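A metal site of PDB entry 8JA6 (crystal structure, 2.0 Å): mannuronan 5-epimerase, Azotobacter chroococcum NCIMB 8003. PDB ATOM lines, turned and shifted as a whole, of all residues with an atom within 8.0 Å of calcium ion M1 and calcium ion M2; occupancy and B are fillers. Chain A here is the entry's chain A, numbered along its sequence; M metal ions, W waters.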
ATOM      1  N   VAL A 330       1.496  39.345 -13.848  1.00  0.00           N
ATOM      2  CA  VAL A 330       0.396  39.026 -12.949  1.00  0.00           C
ATOM      3  C   VAL A 330       0.843  37.889 -12.043  1.00  0.00           C
ATOM      4  O   VAL A 330       0.964  36.747 -12.493  1.00  0.00           O
ATOM      5  CB  VAL A 330      -0.876  38.601 -13.699  1.00  0.00           C
ATOM      6  CG1 VAL A 330      -2.084  38.573 -12.753  1.00  0.00           C
ATOM      7  CG2 VAL A 330      -1.140  39.516 -14.903  1.00  0.00           C
ATOM      8  N   GLY A 332      -0.395  35.735  -9.932  1.00  0.00           N
ATOM      9  CA  GLY A 332      -1.613  35.088  -9.464  1.00  0.00           C
ATOM     10  C   GLY A 332      -2.521  34.795 -10.638  1.00  0.00           C
ATOM     11  O   GLY A 332      -2.184  35.042 -11.793  1.00  0.00           O
ATOM     12  N   ALA A 333      -3.701  34.274 -10.310  1.00  0.00           N
ATOM     13  CA  ALA A 333      -4.595  33.747 -11.334  1.00  0.00           C
ATOM     14  C   ALA A 333      -5.337  34.849 -12.082  1.00  0.00           C
ATOM     15  O   ALA A 333      -5.851  35.803 -11.477  1.00  0.00           O
ATOM     16  CB  ALA A 333      -5.622  32.799 -10.711  1.00  0.00           C
ATOM     17  N   ALA A 334      -5.426  34.688 -13.393  1.00  0.00           N
ATOM     18  CA  ALA A 334      -6.252  35.551 -14.238  1.00  0.00           C
ATOM     19  C   ALA A 334      -7.434  34.757 -14.783  1.00  0.00           C
ATOM     20  O   ALA A 334      -7.260  33.665 -15.337  1.00  0.00           O
ATOM     21  CB  ALA A 334      -5.421  36.142 -15.390  1.00  0.00           C
ATOM     22  N   ASP A 346      -4.134  36.653 -23.151  1.00  0.00           N
ATOM     23  CA  ASP A 346      -2.842  36.134 -22.718  1.00  0.00           C
ATOM     24  C   ASP A 346      -2.832  36.063 -21.196  1.00  0.00           C
ATOM     25  O   ASP A 346      -3.000  37.099 -20.527  1.00  0.00           O
ATOM     26  CB  ASP A 346      -1.688  37.016 -23.201  1.00  0.00           C
ATOM     27  CG  ASP A 346      -1.538  37.035 -24.725  1.00  0.00           C
ATOM     28  OD1 ASP A 346      -0.850  37.955 -25.227  1.00  0.00           O
ATOM     29  OD2 ASP A 346      -2.074  36.143 -25.417  1.00  0.00           O
ATOM     30  N   GLY A 347      -2.642  34.868 -20.649  1.00  0.00           N
ATOM     31  CA  GLY A 347      -2.393  34.728 -19.236  1.00  0.00           C
ATOM     32  C   GLY A 347      -0.966  35.134 -18.887  1.00  0.00           C
ATOM     33  O   GLY A 347      -0.198  35.606 -19.725  1.00  0.00           O
ATOM     34  N   ALA A 348      -0.608  34.929 -17.626  1.00  0.00           N
ATOM     35  CA  ALA A 348       0.685  35.352 -17.087  1.00  0.00           C
ATOM     36  C   ALA A 348       1.198  34.205 -16.212  1.00  0.00           C
ATOM     37  O   ALA A 348       0.878  33.039 -16.450  1.00  0.00           O
ATOM     38  CB  ALA A 348       0.566  36.703 -16.369  1.00  0.00           C
ATOM     39  N   ALA A 349       2.075  34.527 -15.254  1.00  0.00           N
ATOM     40  CA  ALA A 349       2.767  33.498 -14.470  1.00  0.00           C
ATOM     41  C   ALA A 349       1.826  32.643 -13.634  1.00  0.00           C
ATOM     42  O   ALA A 349       2.250  31.582 -13.156  1.00  0.00           O
ATOM     43  CB  ALA A 349       3.814  34.140 -13.554  1.00  0.00           C
ATOM     44  N   GLY A 350       0.560  33.045 -13.431  1.00  0.00           N
ATOM     45  CA  GLY A 350      -0.349  32.293 -12.588  1.00  0.00           C
ATOM     46  C   GLY A 350      -1.044  31.148 -13.331  1.00  0.00           C
ATOM     47  O   GLY A 350      -0.825  30.911 -14.511  1.00  0.00           O
ATOM     48  N   ASN A 351      -1.880  30.424 -12.583  1.00  0.00           N
ATOM     49  CA  ASN A 351      -2.672  29.324 -13.134  1.00  0.00           C
ATOM     50  C   ASN A 351      -3.983  29.950 -13.603  1.00  0.00           C
ATOM     51  O   ASN A 351      -4.870  30.216 -12.787  1.00  0.00           O
ATOM     52  CB  ASN A 351      -2.926  28.223 -12.107  1.00  0.00           C
ATOM     53  CG  ASN A 351      -1.648  27.473 -11.705  1.00  0.00           C
ATOM     54  OD1 ASN A 351      -0.583  27.641 -12.288  1.00  0.00           O
ATOM     55  ND2 ASN A 351      -1.778  26.635 -10.682  1.00  0.00           N
ATOM     56  N   ASP A 352      -4.103  30.187 -14.894  1.00  0.00           N
ATOM     57  CA  ASP A 352      -5.167  31.018 -15.429  1.00  0.00           C
ATOM     58  C   ASP A 352      -6.273  30.198 -16.070  1.00  0.00           C
ATOM     59  O   ASP A 352      -6.080  29.034 -16.432  1.00  0.00           O
ATOM     60  CB  ASP A 352      -4.602  32.022 -16.453  1.00  0.00           C
ATOM     61  CG  ASP A 352      -3.367  32.770 -15.928  1.00  0.00           C
ATOM     62  OD1 ASP A 352      -3.430  33.329 -14.810  1.00  0.00           O
ATOM     63  OD2 ASP A 352      -2.344  32.810 -16.644  1.00  0.00           O
ATOM     64  N   LEU A 353      -7.440  30.820 -16.196  1.00  0.00           N
ATOM     65  CA  LEU A 353      -8.583  30.238 -16.895  1.00  0.00           C
ATOM     66  C   LEU A 353      -8.875  31.117 -18.108  1.00  0.00           C
ATOM     67  O   LEU A 353      -9.078  32.319 -17.959  1.00  0.00           O
ATOM     68  CB  LEU A 353      -9.812  30.164 -15.978  1.00  0.00           C
ATOM     69  CG  LEU A 353     -11.098  29.751 -16.677  1.00  0.00           C
ATOM     70  CD1 LEU A 353     -10.917  28.327 -17.189  1.00  0.00           C
ATOM     71  CD2 LEU A 353     -12.304  29.855 -15.741  1.00  0.00           C
ATOM     72  N   LEU A 354      -8.865  30.524 -19.297  1.00  0.00           N
ATOM     73  CA  LEU A 354      -9.060  31.276 -20.535  1.00  0.00           C
ATOM     74  C   LEU A 354     -10.219  30.704 -21.336  1.00  0.00           C
ATOM     75  O   LEU A 354     -10.257  29.502 -21.595  1.00  0.00           O
ATOM     76  CB  LEU A 354      -7.782  31.250 -21.384  1.00  0.00           C
ATOM     77  CG  LEU A 354      -6.605  31.923 -20.691  1.00  0.00           C
ATOM     78  CD1 LEU A 354      -5.729  30.870 -20.069  1.00  0.00           C
ATOM     79  CD2 LEU A 354      -5.840  32.789 -21.668  1.00  0.00           C
ATOM     80  N   SER A 364      -3.312  32.422 -24.985  1.00  0.00           N
ATOM     81  CA  SER A 364      -2.039  31.924 -24.502  1.00  0.00           C
ATOM     82  C   SER A 364      -2.054  31.898 -22.979  1.00  0.00           C
ATOM     83  O   SER A 364      -2.659  32.753 -22.334  1.00  0.00           O
ATOM     84  CB  SER A 364      -0.874  32.758 -25.042  1.00  0.00           C
ATOM     85  OG  SER A 364      -0.711  33.928 -24.289  1.00  0.00           O
ATOM     86  N   GLY A 365      -1.424  30.887 -22.395  1.00  0.00           N
ATOM     87  CA  GLY A 365      -1.453  30.775 -20.959  1.00  0.00           C
ATOM     88  C   GLY A 365      -0.275  31.408 -20.235  1.00  0.00           C
ATOM     89  O   GLY A 365      -0.386  31.801 -19.067  1.00  0.00           O
ATOM     90  N   GLY A 366       0.871  31.486 -20.908  1.00  0.00           N
ATOM     91  CA  GLY A 366       2.058  31.894 -20.175  1.00  0.00           C
ATOM     92  C   GLY A 366       2.547  30.791 -19.241  1.00  0.00           C
ATOM     93  O   GLY A 366       2.230  29.595 -19.398  1.00  0.00           O
ATOM     94  N   GLY A 367       3.338  31.203 -18.244  1.00  0.00           N
ATOM     95  CA  GLY A 367       3.842  30.279 -17.259  1.00  0.00           C
ATOM     96  C   GLY A 367       2.722  29.713 -16.407  1.00  0.00           C
ATOM     97  O   GLY A 367       1.566  30.153 -16.462  1.00  0.00           O
ATOM     98  N   GLY A 368       3.052  28.694 -15.618  1.00  0.00           N
ATOM     99  CA  GLY A 368       2.069  28.054 -14.774  1.00  0.00           C
ATOM    100  C   GLY A 368       1.171  27.094 -15.539  1.00  0.00           C
ATOM    101  O   GLY A 368       1.350  26.816 -16.724  1.00  0.00           O
ATOM    102  N   ALA A 369       0.184  26.552 -14.828  1.00  0.00           N
ATOM    103  CA  ALA A 369      -0.706  25.524 -15.349  1.00  0.00           C
ATOM    104  C   ALA A 369      -2.054  26.161 -15.652  1.00  0.00           C
ATOM    105  O   ALA A 369      -2.804  26.513 -14.733  1.00  0.00           O
ATOM    106  CB  ALA A 369      -0.838  24.373 -14.347  1.00  0.00           C
ATOM    107  N   ASP A 370      -2.376  26.279 -16.935  1.00  0.00           N
ATOM    108  CA  ASP A 370      -3.542  27.038 -17.375  1.00  0.00           C
ATOM    109  C   ASP A 370      -4.607  26.142 -17.976  1.00  0.00           C
ATOM    110  O   ASP A 370      -4.298  25.120 -18.594  1.00  0.00           O
ATOM    111  CB  ASP A 370      -3.129  28.098 -18.392  1.00  0.00           C
ATOM    112  CG  ASP A 370      -2.018  28.979 -17.870  1.00  0.00           C
ATOM    113  OD1 ASP A 370      -0.915  28.924 -18.429  1.00  0.00           O
ATOM    114  OD2 ASP A 370      -2.248  29.730 -16.891  1.00  0.00           O
ATOM    115  N   THR A 371      -5.864  26.551 -17.813  1.00  0.00           N
ATOM    116  CA  THR A 371      -7.005  25.829 -18.361  1.00  0.00           C
ATOM    117  C   THR A 371      -7.598  26.658 -19.491  1.00  0.00           C
ATOM    118  O   THR A 371      -7.955  27.823 -19.298  1.00  0.00           O
ATOM    119  CB  THR A 371      -8.049  25.543 -17.273  1.00  0.00           C
ATOM    120  OG1 THR A 371      -7.463  24.678 -16.279  1.00  0.00           O
ATOM    121  CG2 THR A 371      -9.240  24.850 -17.847  1.00  0.00           C
ATOM    122  N   PHE A 372      -7.662  26.065 -20.690  1.00  0.00           N
ATOM    123  CA  PHE A 372      -8.298  26.685 -21.843  1.00  0.00           C
ATOM    124  C   PHE A 372      -9.654  26.019 -22.011  1.00  0.00           C
ATOM    125  O   PHE A 372      -9.735  24.846 -22.387  1.00  0.00           O
ATOM    126  CB  PHE A 372      -7.452  26.505 -23.109  1.00  0.00           C
ATOM    127  CG  PHE A 372      -6.069  27.034 -22.973  1.00  0.00           C
ATOM    128  CD1 PHE A 372      -5.787  28.352 -23.340  1.00  0.00           C
ATOM    129  CD2 PHE A 372      -5.032  26.238 -22.486  1.00  0.00           C
ATOM    130  CE1 PHE A 372      -4.494  28.853 -23.204  1.00  0.00           C
ATOM    131  CE2 PHE A 372      -3.752  26.735 -22.346  1.00  0.00           C
ATOM    132  CZ  PHE A 372      -3.468  28.039 -22.725  1.00  0.00           C
ATOM    133  N   ASP A 396       0.504  28.510 -26.894  1.00  0.00           N
ATOM    134  CA  ASP A 396       1.619  27.958 -26.125  1.00  0.00           C
ATOM    135  C   ASP A 396       1.168  26.777 -25.272  1.00  0.00           C
ATOM    136  O   ASP A 396       1.592  26.650 -24.115  1.00  0.00           O
ATOM    137  CB  ASP A 396       2.243  29.029 -25.233  1.00  0.00           C
ATOM    138  CG  ASP A 396       1.254  29.564 -24.182  1.00  0.00           C
ATOM    139  OD1 ASP A 396       0.032  29.314 -24.311  1.00  0.00           O
ATOM    140  OD2 ASP A 396       1.700  30.218 -23.217  1.00  0.00           O
ATOM    141  N   PHE A 397       0.312  25.917 -25.802  1.00  0.00           N
ATOM    142  CA  PHE A 397      -0.162  24.808 -24.991  1.00  0.00           C
ATOM    143  C   PHE A 397       1.003  23.912 -24.578  1.00  0.00           C
ATOM    144  O   PHE A 397       1.789  23.468 -25.414  1.00  0.00           O
ATOM    145  CB  PHE A 397      -1.208  23.956 -25.717  1.00  0.00           C
ATOM    146  CG  PHE A 397      -1.884  22.952 -24.806  1.00  0.00           C
ATOM    147  CD1 PHE A 397      -1.410  21.653 -24.708  1.00  0.00           C
ATOM    148  CD2 PHE A 397      -2.942  23.330 -23.999  1.00  0.00           C
ATOM    149  CE1 PHE A 397      -2.002  20.745 -23.842  1.00  0.00           C
ATOM    150  CE2 PHE A 397      -3.533  22.422 -23.134  1.00  0.00           C
ATOM    151  CZ  PHE A 397      -3.066  21.129 -23.051  1.00  0.00           C
ATOM    152  N   THR A 398       1.089  23.639 -23.287  1.00  0.00           N
ATOM    153  CA  THR A 398       2.202  22.880 -22.704  1.00  0.00           C
ATOM    154  C   THR A 398       1.689  21.557 -22.160  1.00  0.00           C
ATOM    155  O   THR A 398       1.068  21.531 -21.072  1.00  0.00           O
ATOM    156  CB  THR A 398       2.879  23.709 -21.617  1.00  0.00           C
ATOM    157  OG1 THR A 398       3.109  25.040 -22.096  1.00  0.00           O
ATOM    158  CG2 THR A 398       4.211  23.080 -21.217  1.00  0.00           C
ATOM    159  N   ALA A 401       1.295  20.235 -18.299  1.00  0.00           N
ATOM    160  CA  ALA A 401       1.041  21.377 -17.425  1.00  0.00           C
ATOM    161  C   ALA A 401      -0.312  22.018 -17.684  1.00  0.00           C
ATOM    162  O   ALA A 401      -1.091  22.219 -16.739  1.00  0.00           O
ATOM    163  CB  ALA A 401       2.169  22.420 -17.580  1.00  0.00           C
ATOM    164  N   ASP A 402      -0.609  22.362 -18.931  1.00  0.00           N
ATOM    165  CA  ASP A 402      -1.891  22.994 -19.230  1.00  0.00           C
ATOM    166  C   ASP A 402      -3.000  21.950 -19.403  1.00  0.00           C
ATOM    167  O   ASP A 402      -2.756  20.739 -19.447  1.00  0.00           O
ATOM    168  CB  ASP A 402      -1.789  23.863 -20.476  1.00  0.00           C
ATOM    169  CG  ASP A 402      -0.756  24.965 -20.354  1.00  0.00           C
ATOM    170  OD1 ASP A 402      -0.549  25.499 -19.228  1.00  0.00           O
ATOM    171  OD2 ASP A 402      -0.156  25.298 -21.401  1.00  0.00           O
ATOM    172  N   LEU A 403      -4.227  22.449 -19.519  1.00  0.00           N
ATOM    173  CA  LEU A 403      -5.392  21.595 -19.661  1.00  0.00           C
ATOM    174  C   LEU A 403      -6.352  22.232 -20.656  1.00  0.00           C
ATOM    175  O   LEU A 403      -6.575  23.440 -20.623  1.00  0.00           O
ATOM    176  CB  LEU A 403      -6.099  21.398 -18.301  1.00  0.00           C
ATOM    177  CG  LEU A 403      -7.391  20.560 -18.343  1.00  0.00           C
ATOM    178  CD1 LEU A 403      -7.106  19.068 -18.600  1.00  0.00           C
ATOM    179  CD2 LEU A 403      -8.203  20.746 -17.056  1.00  0.00           C
ATOM    180  N   THR A 476      -6.659  22.850 -13.434  1.00  0.00           N
ATOM    181  CA  THR A 476      -5.449  23.492 -12.947  1.00  0.00           C
ATOM    182  C   THR A 476      -5.713  24.726 -12.093  1.00  0.00           C
ATOM    183  O   THR A 476      -4.784  25.210 -11.427  1.00  0.00           O
ATOM    184  CB  THR A 476      -4.539  23.884 -14.117  1.00  0.00           C
ATOM    185  OG1 THR A 476      -5.102  25.005 -14.813  1.00  0.00           O
ATOM    186  CG2 THR A 476      -4.336  22.728 -15.081  1.00  0.00           C
HETATM  187 CA    CA M   1      -0.530  31.290 -16.850  1.00  0.00          CA
HETATM  188 CA    CA M   2       0.914  27.590 -19.030  1.00  0.00          CA
HETATM  189  O   HOH W   1       2.992  26.294 -19.383  1.00  0.00           O
HETATM  190  O   HOH W   2       0.232  27.810 -21.528  1.00  0.00           O
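OD1 of Asp 352 sits at hydrogen-bond distance from N of Ala 334. The backbone carbonyl oxygen of Asp 370 sits at hydrogen-bond distance from the backbone NH of Leu 403 (2.8 Å). The side-chain carboxylate (OD2) of Asp 396 is in hydrogen-bond range of the backbone NH (N) of Gly 366, at 2.8 Å. The backbone NH of Gly 365 is in hydrogen-bond range of the side-chain carboxylate of Asp 396 (2.9 Å). N of Thr 371 lies within hydrogen-bond range of O of Asp 352, 2.8 Å away. OD2 of Asp 402 lies within hydrogen-bond range of N of Thr 398, at 2.8 Å.
Seven residues have an atom within 4 Å of calcium ion M1: Ala 348, Gly 350, Asp 352, Gly 365, Gly 366, Gly 367 and Asp 370. Along chain A the residues within 4 Å of calcium ion M1 span positions 348 to 370.
Five residues have an atom within 4 Å of calcium ion M2: Gly 366, Gly 367, Gly 368, Asp 370 and Asp 402.
The backbone carbonyl oxygen (O) of Gly 365 is bound to calcium ion M1, at 2.3 Å. Calcium ion M1 is bound by O of Ala 348, at 2.3 Å. The side-chain carboxylate (OD2) of Asp 370 binds calcium ion M1 (2.3 Å). OD2 of Asp 352 binds calcium ion M1, at 2.4 Å. O of Gly 350 binds calcium ion M1 (2.4 Å). Calcium ion M1 is bound by O of Gly 367 (2.4 Å). The side-chain carboxylate (OD1) of Asp 370 is bound to calcium ion M1. Calcium ion M1 has seven donor atoms within binding distance.
Calcium ion M2 is bound by OD1 of Asp 370. The backbone carbonyl oxygen (O) of Gly 366 binds calcium ion M2, at 2.4 Å. O of Gly 368 binds calcium ion M2 (2.5 Å). Water W1 is bound to calcium ion M2, at 2.5 Å. The side-chain carboxylate (OD1) of Asp 402 is bound to calcium ion M2, 2.6 Å away. Water W2 is bound to calcium ion M2 (2.6 Å). Calcium ion M2 has six donor atoms within binding distance.
Water W2 bridges OD2 of Asp 402 and O of Asp 396.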
